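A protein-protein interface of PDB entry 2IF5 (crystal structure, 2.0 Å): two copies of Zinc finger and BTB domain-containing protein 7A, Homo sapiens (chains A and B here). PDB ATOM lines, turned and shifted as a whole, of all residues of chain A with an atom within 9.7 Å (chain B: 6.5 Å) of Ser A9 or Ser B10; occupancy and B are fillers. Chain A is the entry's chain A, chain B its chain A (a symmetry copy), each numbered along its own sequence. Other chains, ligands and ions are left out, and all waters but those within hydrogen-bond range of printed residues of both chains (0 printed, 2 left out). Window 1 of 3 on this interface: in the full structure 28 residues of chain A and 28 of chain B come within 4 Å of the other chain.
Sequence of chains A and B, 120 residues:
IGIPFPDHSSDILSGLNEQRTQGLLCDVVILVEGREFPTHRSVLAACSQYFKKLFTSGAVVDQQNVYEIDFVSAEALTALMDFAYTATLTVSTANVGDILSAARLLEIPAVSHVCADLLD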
ATOM      1  N   PRO A   4       2.807   6.980   1.888  1.00  0.00           N
ATOM      2  CA  PRO A   4       3.936   6.184   1.461  1.00  0.00           C
ATOM      3  C   PRO A   4       3.488   5.071   0.514  1.00  0.00           C
ATOM      4  O   PRO A   4       2.457   4.421   0.768  1.00  0.00           O
ATOM      5  CB  PRO A   4       4.439   5.569   2.783  1.00  0.00           C
ATOM      6  CG  PRO A   4       3.255   5.581   3.708  1.00  0.00           C
ATOM      7  CD  PRO A   4       2.236   6.506   3.171  1.00  0.00           C
ATOM      8  N   PHE A   5       4.275   4.849  -0.531  1.00  0.00           N
ATOM      9  CA  PHE A   5       4.068   3.762  -1.523  1.00  0.00           C
ATOM     10  C   PHE A   5       5.256   2.788  -1.465  1.00  0.00           C
ATOM     11  O   PHE A   5       6.231   2.904  -2.231  1.00  0.00           O
ATOM     12  CB  PHE A   5       3.894   4.309  -2.947  1.00  0.00           C
ATOM     13  CG  PHE A   5       2.623   5.093  -3.138  1.00  0.00           C
ATOM     14  CD1 PHE A   5       2.479   6.365  -2.589  1.00  0.00           C
ATOM     15  CD2 PHE A   5       1.553   4.539  -3.844  1.00  0.00           C
ATOM     16  CE1 PHE A   5       1.298   7.105  -2.782  1.00  0.00           C
ATOM     17  CE2 PHE A   5       0.369   5.258  -4.027  1.00  0.00           C
ATOM     18  CZ  PHE A   5       0.235   6.542  -3.487  1.00  0.00           C
ATOM     19  N   PRO A   6       5.160   1.788  -0.579  1.00  0.00           N
ATOM     20  CA  PRO A   6       6.301   0.898  -0.435  1.00  0.00           C
ATOM     21  C   PRO A   6       6.635   0.036  -1.651  1.00  0.00           C
ATOM     22  O   PRO A   6       7.708  -0.554  -1.664  1.00  0.00           O
ATOM     23  CB  PRO A   6       5.923  -0.035   0.728  1.00  0.00           C
ATOM     24  CG  PRO A   6       4.595   0.437   1.233  1.00  0.00           C
ATOM     25  CD  PRO A   6       4.023   1.434   0.300  1.00  0.00           C
ATOM     26  N   ASP A   7       5.750  -0.037  -2.639  1.00  0.00           N
ATOM     27  CA  ASP A   7       6.035  -0.867  -3.854  1.00  0.00           C
ATOM     28  C   ASP A   7       6.503  -0.020  -5.043  1.00  0.00           C
ATOM     29  O   ASP A   7       6.936  -0.567  -6.039  1.00  0.00           O
ATOM     30  CB  ASP A   7       4.807  -1.665  -4.286  1.00  0.00           C
ATOM     31  CG  ASP A   7       5.180  -2.854  -5.200  1.00  0.00           C
ATOM     32  OD1 ASP A   7       4.477  -3.165  -6.204  1.00  0.00           O
ATOM     33  OD2 ASP A   7       6.193  -3.450  -4.889  1.00  0.00           O
ATOM     34  N   HIS A   8       6.423   1.310  -4.910  1.00  0.00           N
ATOM     35  CA  HIS A   8       6.693   2.237  -6.005  1.00  0.00           C
ATOM     36  C   HIS A   8       8.099   2.163  -6.599  1.00  0.00           C
ATOM     37  O   HIS A   8       8.225   2.174  -7.803  1.00  0.00           O
ATOM     38  CB  HIS A   8       6.350   3.695  -5.636  1.00  0.00           C
ATOM     39  CG  HIS A   8       6.680   4.681  -6.715  1.00  0.00           C
ATOM     40  ND1 HIS A   8       5.935   4.796  -7.862  1.00  0.00           N
ATOM     41  CD2 HIS A   8       7.703   5.571  -6.838  1.00  0.00           C
ATOM     42  CE1 HIS A   8       6.451   5.741  -8.631  1.00  0.00           C
ATOM     43  NE2 HIS A   8       7.521   6.232  -8.028  1.00  0.00           N
ATOM     44  N   SER A   9       9.162   2.142  -5.783  1.00  0.00           N
ATOM     45  CA  SER A   9      10.495   2.133  -6.389  1.00  0.00           C
ATOM     46  C   SER A   9      10.731   0.860  -7.192  1.00  0.00           C
ATOM     47  O   SER A   9      11.359   0.910  -8.230  1.00  0.00           O
ATOM     48  CB  SER A   9      11.621   2.309  -5.350  1.00  0.00           C
ATOM     49  OG  SER A   9      11.609   1.238  -4.416  1.00  0.00           O
ATOM     50  N   SER A  10      10.200  -0.264  -6.732  1.00  0.00           N
ATOM     51  CA  SER A  10      10.383  -1.506  -7.457  1.00  0.00           C
ATOM     52  C   SER A  10       9.514  -1.488  -8.714  1.00  0.00           C
ATOM     53  O   SER A  10       9.934  -2.039  -9.700  1.00  0.00           O
ATOM     54  CB  SER A  10      10.086  -2.756  -6.589  1.00  0.00           C
ATOM     55  OG  SER A  10       8.776  -2.601  -6.088  1.00  0.00           O
ATOM     56  N   ASP A  11       8.329  -0.862  -8.672  1.00  0.00           N
ATOM     57  CA  ASP A  11       7.492  -0.690  -9.869  1.00  0.00           C
ATOM     58  C   ASP A  11       8.164   0.204 -10.887  1.00  0.00           C
ATOM     59  O   ASP A  11       8.160  -0.113 -12.089  1.00  0.00           O
ATOM     60  CB  ASP A  11       6.106  -0.099  -9.527  1.00  0.00           C
ATOM     61  CG  ASP A  11       5.167  -1.149  -8.907  1.00  0.00           C
ATOM     62  OD1 ASP A  11       5.349  -2.374  -9.103  1.00  0.00           O
ATOM     63  OD2 ASP A  11       4.245  -0.773  -8.209  1.00  0.00           O
ATOM     64  N   ILE A  12       8.783   1.286 -10.426  1.00  0.00           N
ATOM     65  CA  ILE A  12       9.635   2.116 -11.311  1.00  0.00           C
ATOM     66  C   ILE A  12      10.745   1.301 -11.949  1.00  0.00           C
ATOM     67  O   ILE A  12      10.943   1.376 -13.164  1.00  0.00           O
ATOM     68  CB  ILE A  12      10.260   3.368 -10.588  1.00  0.00           C
ATOM     69  CG1 ILE A  12       9.176   4.400 -10.299  1.00  0.00           C
ATOM     70  CG2 ILE A  12      11.339   4.007 -11.469  1.00  0.00           C
ATOM     71  CD1 ILE A  12       8.481   4.938 -11.562  1.00  0.00           C
ATOM     72  N   LEU A  13      11.453   0.507 -11.135  1.00  0.00           N
ATOM     73  CA  LEU A  13      12.587  -0.228 -11.660  1.00  0.00           C
ATOM     74  C   LEU A  13      12.138  -1.261 -12.703  1.00  0.00           C
ATOM     75  O   LEU A  13      12.799  -1.467 -13.741  1.00  0.00           O
ATOM     76  CB  LEU A  13      13.382  -0.895 -10.532  1.00  0.00           C
ATOM     77  CG  LEU A  13      14.769  -1.363 -10.964  1.00  0.00           C
ATOM     78  CD1 LEU A  13      15.677  -0.215 -11.388  1.00  0.00           C
ATOM     79  CD2 LEU A  13      15.359  -2.162  -9.824  1.00  0.00           C
ATOM     80  N   SER A  14      11.020  -1.926 -12.410  1.00  0.00           N
ATOM     81  CA  SER A  14      10.413  -2.833 -13.337  1.00  0.00           C
ATOM     82  C   SER A  14      10.100  -2.175 -14.683  1.00  0.00           C
ATOM     83  O   SER A  14      10.250  -2.789 -15.748  1.00  0.00           O
ATOM     84  CB  SER A  14       9.108  -3.351 -12.712  1.00  0.00           C
ATOM     85  OG  SER A  14       8.662  -4.457 -13.448  1.00  0.00           O
ATOM     86  N   GLY A  15       9.570  -0.956 -14.636  1.00  0.00           N
ATOM     87  CA  GLY A  15       9.251  -0.220 -15.825  1.00  0.00           C
ATOM     88  C   GLY A  15      10.491   0.119 -16.601  1.00  0.00           C
ATOM     89  O   GLY A  15      10.502   0.001 -17.812  1.00  0.00           O
ATOM     90  N   LEU A  16      11.576   0.467 -15.907  1.00  0.00           N
ATOM     91  CA  LEU A  16      12.830   0.798 -16.582  1.00  0.00           C
ATOM     92  C   LEU A  16      13.416  -0.473 -17.199  1.00  0.00           C
ATOM     93  O   LEU A  16      13.956  -0.438 -18.312  1.00  0.00           O
ATOM     94  CB  LEU A  16      13.833   1.480 -15.610  1.00  0.00           C
ATOM     95  CG  LEU A  16      13.369   2.815 -15.034  1.00  0.00           C
ATOM     96  CD1 LEU A  16      14.228   3.265 -13.826  1.00  0.00           C
ATOM     97  CD2 LEU A  16      13.444   3.866 -16.129  1.00  0.00           C
ATOM     98  N   ASN A  17      13.297  -1.588 -16.479  1.00  0.00           N
ATOM     99  CA  ASN A  17      13.716  -2.889 -17.016  1.00  0.00           C
ATOM    100  C   ASN A  17      12.894  -3.287 -18.270  1.00  0.00           C
ATOM    101  O   ASN A  17      13.442  -3.809 -19.217  1.00  0.00           O
ATOM    102  CB  ASN A  17      13.593  -3.967 -15.947  1.00  0.00           C
ATOM    103  CG  ASN A  17      14.313  -5.251 -16.324  1.00  0.00           C
ATOM    104  OD1 ASN A  17      13.809  -6.352 -16.090  1.00  0.00           O
ATOM    105  ND2 ASN A  17      15.462  -5.109 -16.928  1.00  0.00           N
ATOM    106  N   ALA A  46      23.021   6.229 -11.480  1.00  0.00           N
ATOM    107  CA  ALA A  46      22.435   6.098 -10.137  1.00  0.00           C
ATOM    108  C   ALA A  46      23.029   4.935  -9.343  1.00  0.00           C
ATOM    109  O   ALA A  46      22.930   4.895  -8.115  1.00  0.00           O
ATOM    110  CB  ALA A  46      20.903   5.930 -10.256  1.00  0.00           C
ATOM    111  N   CYS A  47      23.639   3.976 -10.013  1.00  0.00           N
ATOM    112  CA  CYS A  47      24.279   2.901  -9.231  1.00  0.00           C
ATOM    113  C   CYS A  47      25.743   2.628  -9.429  1.00  0.00           C
ATOM    114  O   CYS A  47      26.285   1.754  -8.755  1.00  0.00           O
ATOM    115  CB  CYS A  47      23.511   1.586  -9.313  1.00  0.00           C
ATOM    116  SG  CYS A  47      23.670   0.681 -10.811  1.00  0.00           S
ATOM    117  N   ALA A  84      21.418  -4.053 -11.801  1.00  0.00           N
ATOM    118  CA  ALA A  84      21.060  -2.619 -11.790  1.00  0.00           C
ATOM    119  C   ALA A  84      19.569  -2.440 -12.021  1.00  0.00           C
ATOM    120  O   ALA A  84      18.900  -1.634 -11.352  1.00  0.00           O
ATOM    121  CB  ALA A  84      21.846  -1.860 -12.868  1.00  0.00           C
ATOM    122  N   TYR A  85      19.044  -3.238 -12.945  1.00  0.00           N
ATOM    123  CA  TYR A  85      17.670  -3.094 -13.390  1.00  0.00           C
ATOM    124  C   TYR A  85      16.663  -4.014 -12.707  1.00  0.00           C
ATOM    125  O   TYR A  85      15.474  -3.924 -12.968  1.00  0.00           O
ATOM    126  CB  TYR A  85      17.628  -3.377 -14.869  1.00  0.00           C
ATOM    127  CG  TYR A  85      17.997  -2.189 -15.695  1.00  0.00           C
ATOM    128  CD1 TYR A  85      19.352  -1.945 -16.050  1.00  0.00           C
ATOM    129  CD2 TYR A  85      17.012  -1.299 -16.143  1.00  0.00           C
ATOM    130  CE1 TYR A  85      19.710  -0.854 -16.846  1.00  0.00           C
ATOM    131  CE2 TYR A  85      17.368  -0.193 -16.951  1.00  0.00           C
ATOM    132  CZ  TYR A  85      18.712   0.015 -17.287  1.00  0.00           C
ATOM    133  OH  TYR A  85      19.090   1.086 -18.078  1.00  0.00           O
ATOM    134  N   THR A  86      17.114  -4.923 -11.852  1.00  0.00           N
ATOM    135  CA  THR A  86      16.173  -5.843 -11.164  1.00  0.00           C
ATOM    136  C   THR A  86      16.340  -5.951  -9.626  1.00  0.00           C
ATOM    137  O   THR A  86      15.452  -6.498  -8.950  1.00  0.00           O
ATOM    138  CB  THR A  86      16.261  -7.244 -11.711  1.00  0.00           C
ATOM    139  OG1 THR A  86      17.535  -7.810 -11.338  1.00  0.00           O
ATOM    140  CG2 THR A  86      16.114  -7.238 -13.279  1.00  0.00           C
ATOM    141  N   ALA A  87      17.465  -5.481  -9.073  1.00  0.00           N
ATOM    142  CA  ALA A  87      17.734  -5.661  -7.620  1.00  0.00           C
ATOM    143  C   ALA A  87      18.064  -7.107  -7.177  1.00  0.00           C
ATOM    144  O   ALA A  87      17.944  -7.474  -5.991  1.00  0.00           O
ATOM    145  CB  ALA A  87      16.574  -5.119  -6.794  1.00  0.00           C
ATOM    146  N   PRO B   6      17.218  -5.829  -1.187  1.00  0.00           N
ATOM    147  CA  PRO B   6      15.946  -5.181  -0.913  1.00  0.00           C
ATOM    148  C   PRO B   6      15.974  -3.655  -0.843  1.00  0.00           C
ATOM    149  O   PRO B   6      14.905  -3.058  -0.843  1.00  0.00           O
ATOM    150  CB  PRO B   6      15.522  -5.719   0.463  1.00  0.00           C
ATOM    151  CG  PRO B   6      16.565  -6.717   0.865  1.00  0.00           C
ATOM    152  CD  PRO B   6      17.721  -6.640  -0.056  1.00  0.00           C
ATOM    153  N   ASP B   7      17.151  -3.045  -0.783  1.00  0.00           N
ATOM    154  CA  ASP B   7      17.228  -1.549  -0.717  1.00  0.00           C
ATOM    155  C   ASP B   7      17.564  -0.920  -2.075  1.00  0.00           C
ATOM    156  O   ASP B   7      17.491   0.284  -2.216  1.00  0.00           O
ATOM    157  CB  ASP B   7      18.273  -1.088   0.297  1.00  0.00           C
ATOM    158  CG  ASP B   7      18.051   0.378   0.733  1.00  0.00           C
ATOM    159  OD1 ASP B   7      19.019   1.175   0.898  1.00  0.00           O
ATOM    160  OD2 ASP B   7      16.890   0.702   0.891  1.00  0.00           O
ATOM    161  N   HIS B   8      17.914  -1.757  -3.061  1.00  0.00           N
ATOM    162  CA  HIS B   8      18.398  -1.298  -4.359  1.00  0.00           C
ATOM    163  C   HIS B   8      17.430  -0.420  -5.152  1.00  0.00           C
ATOM    164  O   HIS B   8      17.853   0.578  -5.690  1.00  0.00           O
ATOM    165  CB  HIS B   8      18.903  -2.459  -5.240  1.00  0.00           C
ATOM    166  CG  HIS B   8      19.344  -2.029  -6.606  1.00  0.00           C
ATOM    167  ND1 HIS B   8      20.520  -1.354  -6.823  1.00  0.00           N
ATOM    168  CD2 HIS B   8      18.745  -2.143  -7.823  1.00  0.00           C
ATOM    169  CE1 HIS B   8      20.655  -1.105  -8.115  1.00  0.00           C
ATOM    170  NE2 HIS B   8      19.592  -1.580  -8.745  1.00  0.00           N
ATOM    171  N   SER B   9      16.151  -0.797  -5.280  1.00  0.00           N
ATOM    172  CA  SER B   9      15.266   0.036  -6.098  1.00  0.00           C
ATOM    173  C   SER B   9      15.092   1.423  -5.491  1.00  0.00           C
ATOM    174  O   SER B   9      15.020   2.394  -6.215  1.00  0.00           O
ATOM    175  CB  SER B   9      13.884  -0.609  -6.326  1.00  0.00           C
ATOM    176  OG  SER B   9      13.211  -0.796  -5.088  1.00  0.00           O
ATOM    177  N   SER B  10      15.061   1.514  -4.168  1.00  0.00           N
ATOM    178  CA  SER B  10      14.905   2.807  -3.531  1.00  0.00           C
ATOM    179  C   SER B  10      16.211   3.591  -3.658  1.00  0.00           C
ATOM    180  O   SER B  10      16.143   4.788  -3.787  1.00  0.00           O
ATOM    181  CB  SER B  10      14.462   2.696  -2.050  1.00  0.00           C
ATOM    182  OG  SER B  10      15.409   1.876  -1.402  1.00  0.00           O
ATOM    183  N   ASP B  11      17.373   2.922  -3.627  1.00  0.00           N
ATOM    184  CA  ASP B  11      18.664   3.583  -3.869  1.00  0.00           C
ATOM    185  C   ASP B  11      18.760   4.101  -5.287  1.00  0.00           C
ATOM    186  O   ASP B  11      19.212   5.239  -5.502  1.00  0.00           O
ATOM    187  CB  ASP B  11      19.858   2.640  -3.602  1.00  0.00           C
ATOM    188  CG  ASP B  11      20.126   2.459  -2.097  1.00  0.00           C
ATOM    189  OD1 ASP B  11      19.744   3.316  -1.265  1.00  0.00           O
ATOM    190  OD2 ASP B  11      20.710   1.461  -1.721  1.00  0.00           O
ATOM    191  N   ILE B  12      18.300   3.310  -6.250  1.00  0.00           N
ATOM    192  CA  ILE B  12      18.167   3.800  -7.644  1.00  0.00           C
ATOM    193  C   ILE B  12      17.284   5.031  -7.725  1.00  0.00           C
ATOM    194  O   ILE B  12      17.667   6.023  -8.351  1.00  0.00           O
ATOM    195  CB  ILE B  12      17.630   2.708  -8.645  1.00  0.00           C
ATOM    196  CG1 ILE B  12      18.699   1.650  -8.888  1.00  0.00           C
ATOM    197  CG2 ILE B  12      17.251   3.355  -9.982  1.00  0.00           C
ATOM    198  CD1 ILE B  12      19.990   2.206  -9.513  1.00  0.00           C
ATOM    199  N   LEU B  13      16.114   4.978  -7.075  1.00  0.00           N
ATOM    200  CA  LEU B  13      15.181   6.082  -7.186  1.00  0.00           C
ATOM    201  C   LEU B  13      15.763   7.359  -6.566  1.00  0.00           C
ATOM    202  O   LEU B  13      15.598   8.475  -7.099  1.00  0.00           O
ATOM    203  CB  LEU B  13      13.830   5.728  -6.553  1.00  0.00           C
ATOM    204  CG  LEU B  13      12.707   6.679  -6.956  1.00  0.00           C
ATOM    205  CD1 LEU B  13      12.404   6.642  -8.448  1.00  0.00           C
ATOM    206  CD2 LEU B  13      11.494   6.335  -6.122  1.00  0.00           C
ATOM    207  N   SER B  14      16.428   7.192  -5.423  1.00  0.00           N
ATOM    208  CA  SER B  14      17.128   8.268  -4.788  1.00  0.00           C
ATOM    209  C   SER B  14      18.156   8.925  -5.711  1.00  0.00           C
ATOM    210  O   SER B  14      18.339  10.150  -5.701  1.00  0.00           O
ATOM    211  CB  SER B  14      17.844   7.707  -3.550  1.00  0.00           C
ATOM    212  OG  SER B  14      18.270   8.776  -2.751  1.00  0.00           O
ATOM    213  N   GLY B  15      18.902   8.103  -6.444  1.00  0.00           N
ATOM    214  CA  GLY B  15      19.887   8.590  -7.366  1.00  0.00           C
ATOM    215  C   GLY B  15      19.247   9.351  -8.490  1.00  0.00           C
ATOM    216  O   GLY B  15      19.740  10.395  -8.876  1.00  0.00           O
ATOM    217  N   ALA B  87       8.504   8.032  -4.072  1.00  0.00           N
ATOM    218  CA  ALA B  87       7.587   7.023  -3.474  1.00  0.00           C
ATOM    219  C   ALA B  87       6.740   7.519  -2.277  1.00  0.00           C
ATOM    220  O   ALA B  87       6.229   6.727  -1.461  1.00  0.00           O
ATOM    221  CB  ALA B  87       8.362   5.772  -3.076  1.00  0.00           C
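Ser A9 touches just these residues of chain B: Ser B9 (2.7 Å) and Ser B10 (3.5 Å). Ser B10 touches just one residue of chain A: Ser A9. No residue of chain A comes within 4 Å of Asp B7. Of chain A, only Ser A9 (2.7 Å) and Ser A10 (3.5 Å) come within 4 Å of Ser B9. Of chain A, only His A8 (3.9 Å) comes within 4 Å of Leu B13. Printed residues of chain B within 4 Å of Pro A4: Ala B87 (3.8 Å). Printed residues of chain A within 4 Å of His B8: Leu A13 (3.9 Å), Ala A84 (2.7 Å) and Ala A87 (3.7 Å). Of the printed residues of chain B, Ser A10 touches Ser B9 (3.5 Å). Gly B15 touches none of the printed residues of chain A. The nearest residue of chain B that does not touch Ser A9 is Leu B13 (4.1 Å). The nearest printed residue of chain A that does not touch Ile B12 is Ala A84 (4.1 Å).
Of the 11 printed residues of chain B, 6 touch a printed residue of chain A. Printed residues of chain B that touch a printed residue of chain A: His B8, Ser B9, Ser B10, Ile B12, Leu B13 and Ala B87.
The backbone NH of Phe A5 is in hydrogen-bond range of the backbone carbonyl oxygen of Ala B87 (2.9 Å). The side-chain hydroxyl (OG) of Ser B9 sits at hydrogen-bond distance from the side-chain hydroxyl (OG) of Ser A9, at 2.7 Å. The backbone NH of Ser B10 lies within hydrogen-bond range of the side-chain hydroxyl of Ser A9. N of Ser A10 sits at hydrogen-bond distance from OG of Ser B9, at 3.5 Å. O of Ala A84 sits at hydrogen-bond distance from NE2 of His B8.
The side-chain hydroxyl (OG) of Ser A10 sits at hydrogen-bond distance from the backbone carbonyl oxygen (O) of Asp A7, at 2.7 Å. The side-chain hydroxyl (OG) of Ser B10 lies within hydrogen-bond range of the backbone carbonyl oxygen (O) of Asp B7.
Among the printed residues, merely in contact across the chains: Pro A4 with Ala B87 (3.8 Å), His A8 with Leu B13 (3.9 Å), His A8 with Ala B87 (3.7 Å), Leu A13 with His B8 (3.9 Å), Ala A46 with Ile B12 (3.8 Å), Cys A47 with Ile B12 (3.6 Å) and Ala A87 with His B8 (3.7 Å).
His A8 touches Leu B13, and with the chains exchanged Leu A13 touches His B8. His A8 touches Ala B87, and with the chains exchanged Ala A87 touches His B8. Ser B9 touches its own counterpart, Ser A9. Ser A9 touches Ser B10, and with the chains exchanged Ser A10 touches Ser B9. Of the 12 pairs that touch across the chains among the printed residues, 7 have their exchanged pair printed and touching as well.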
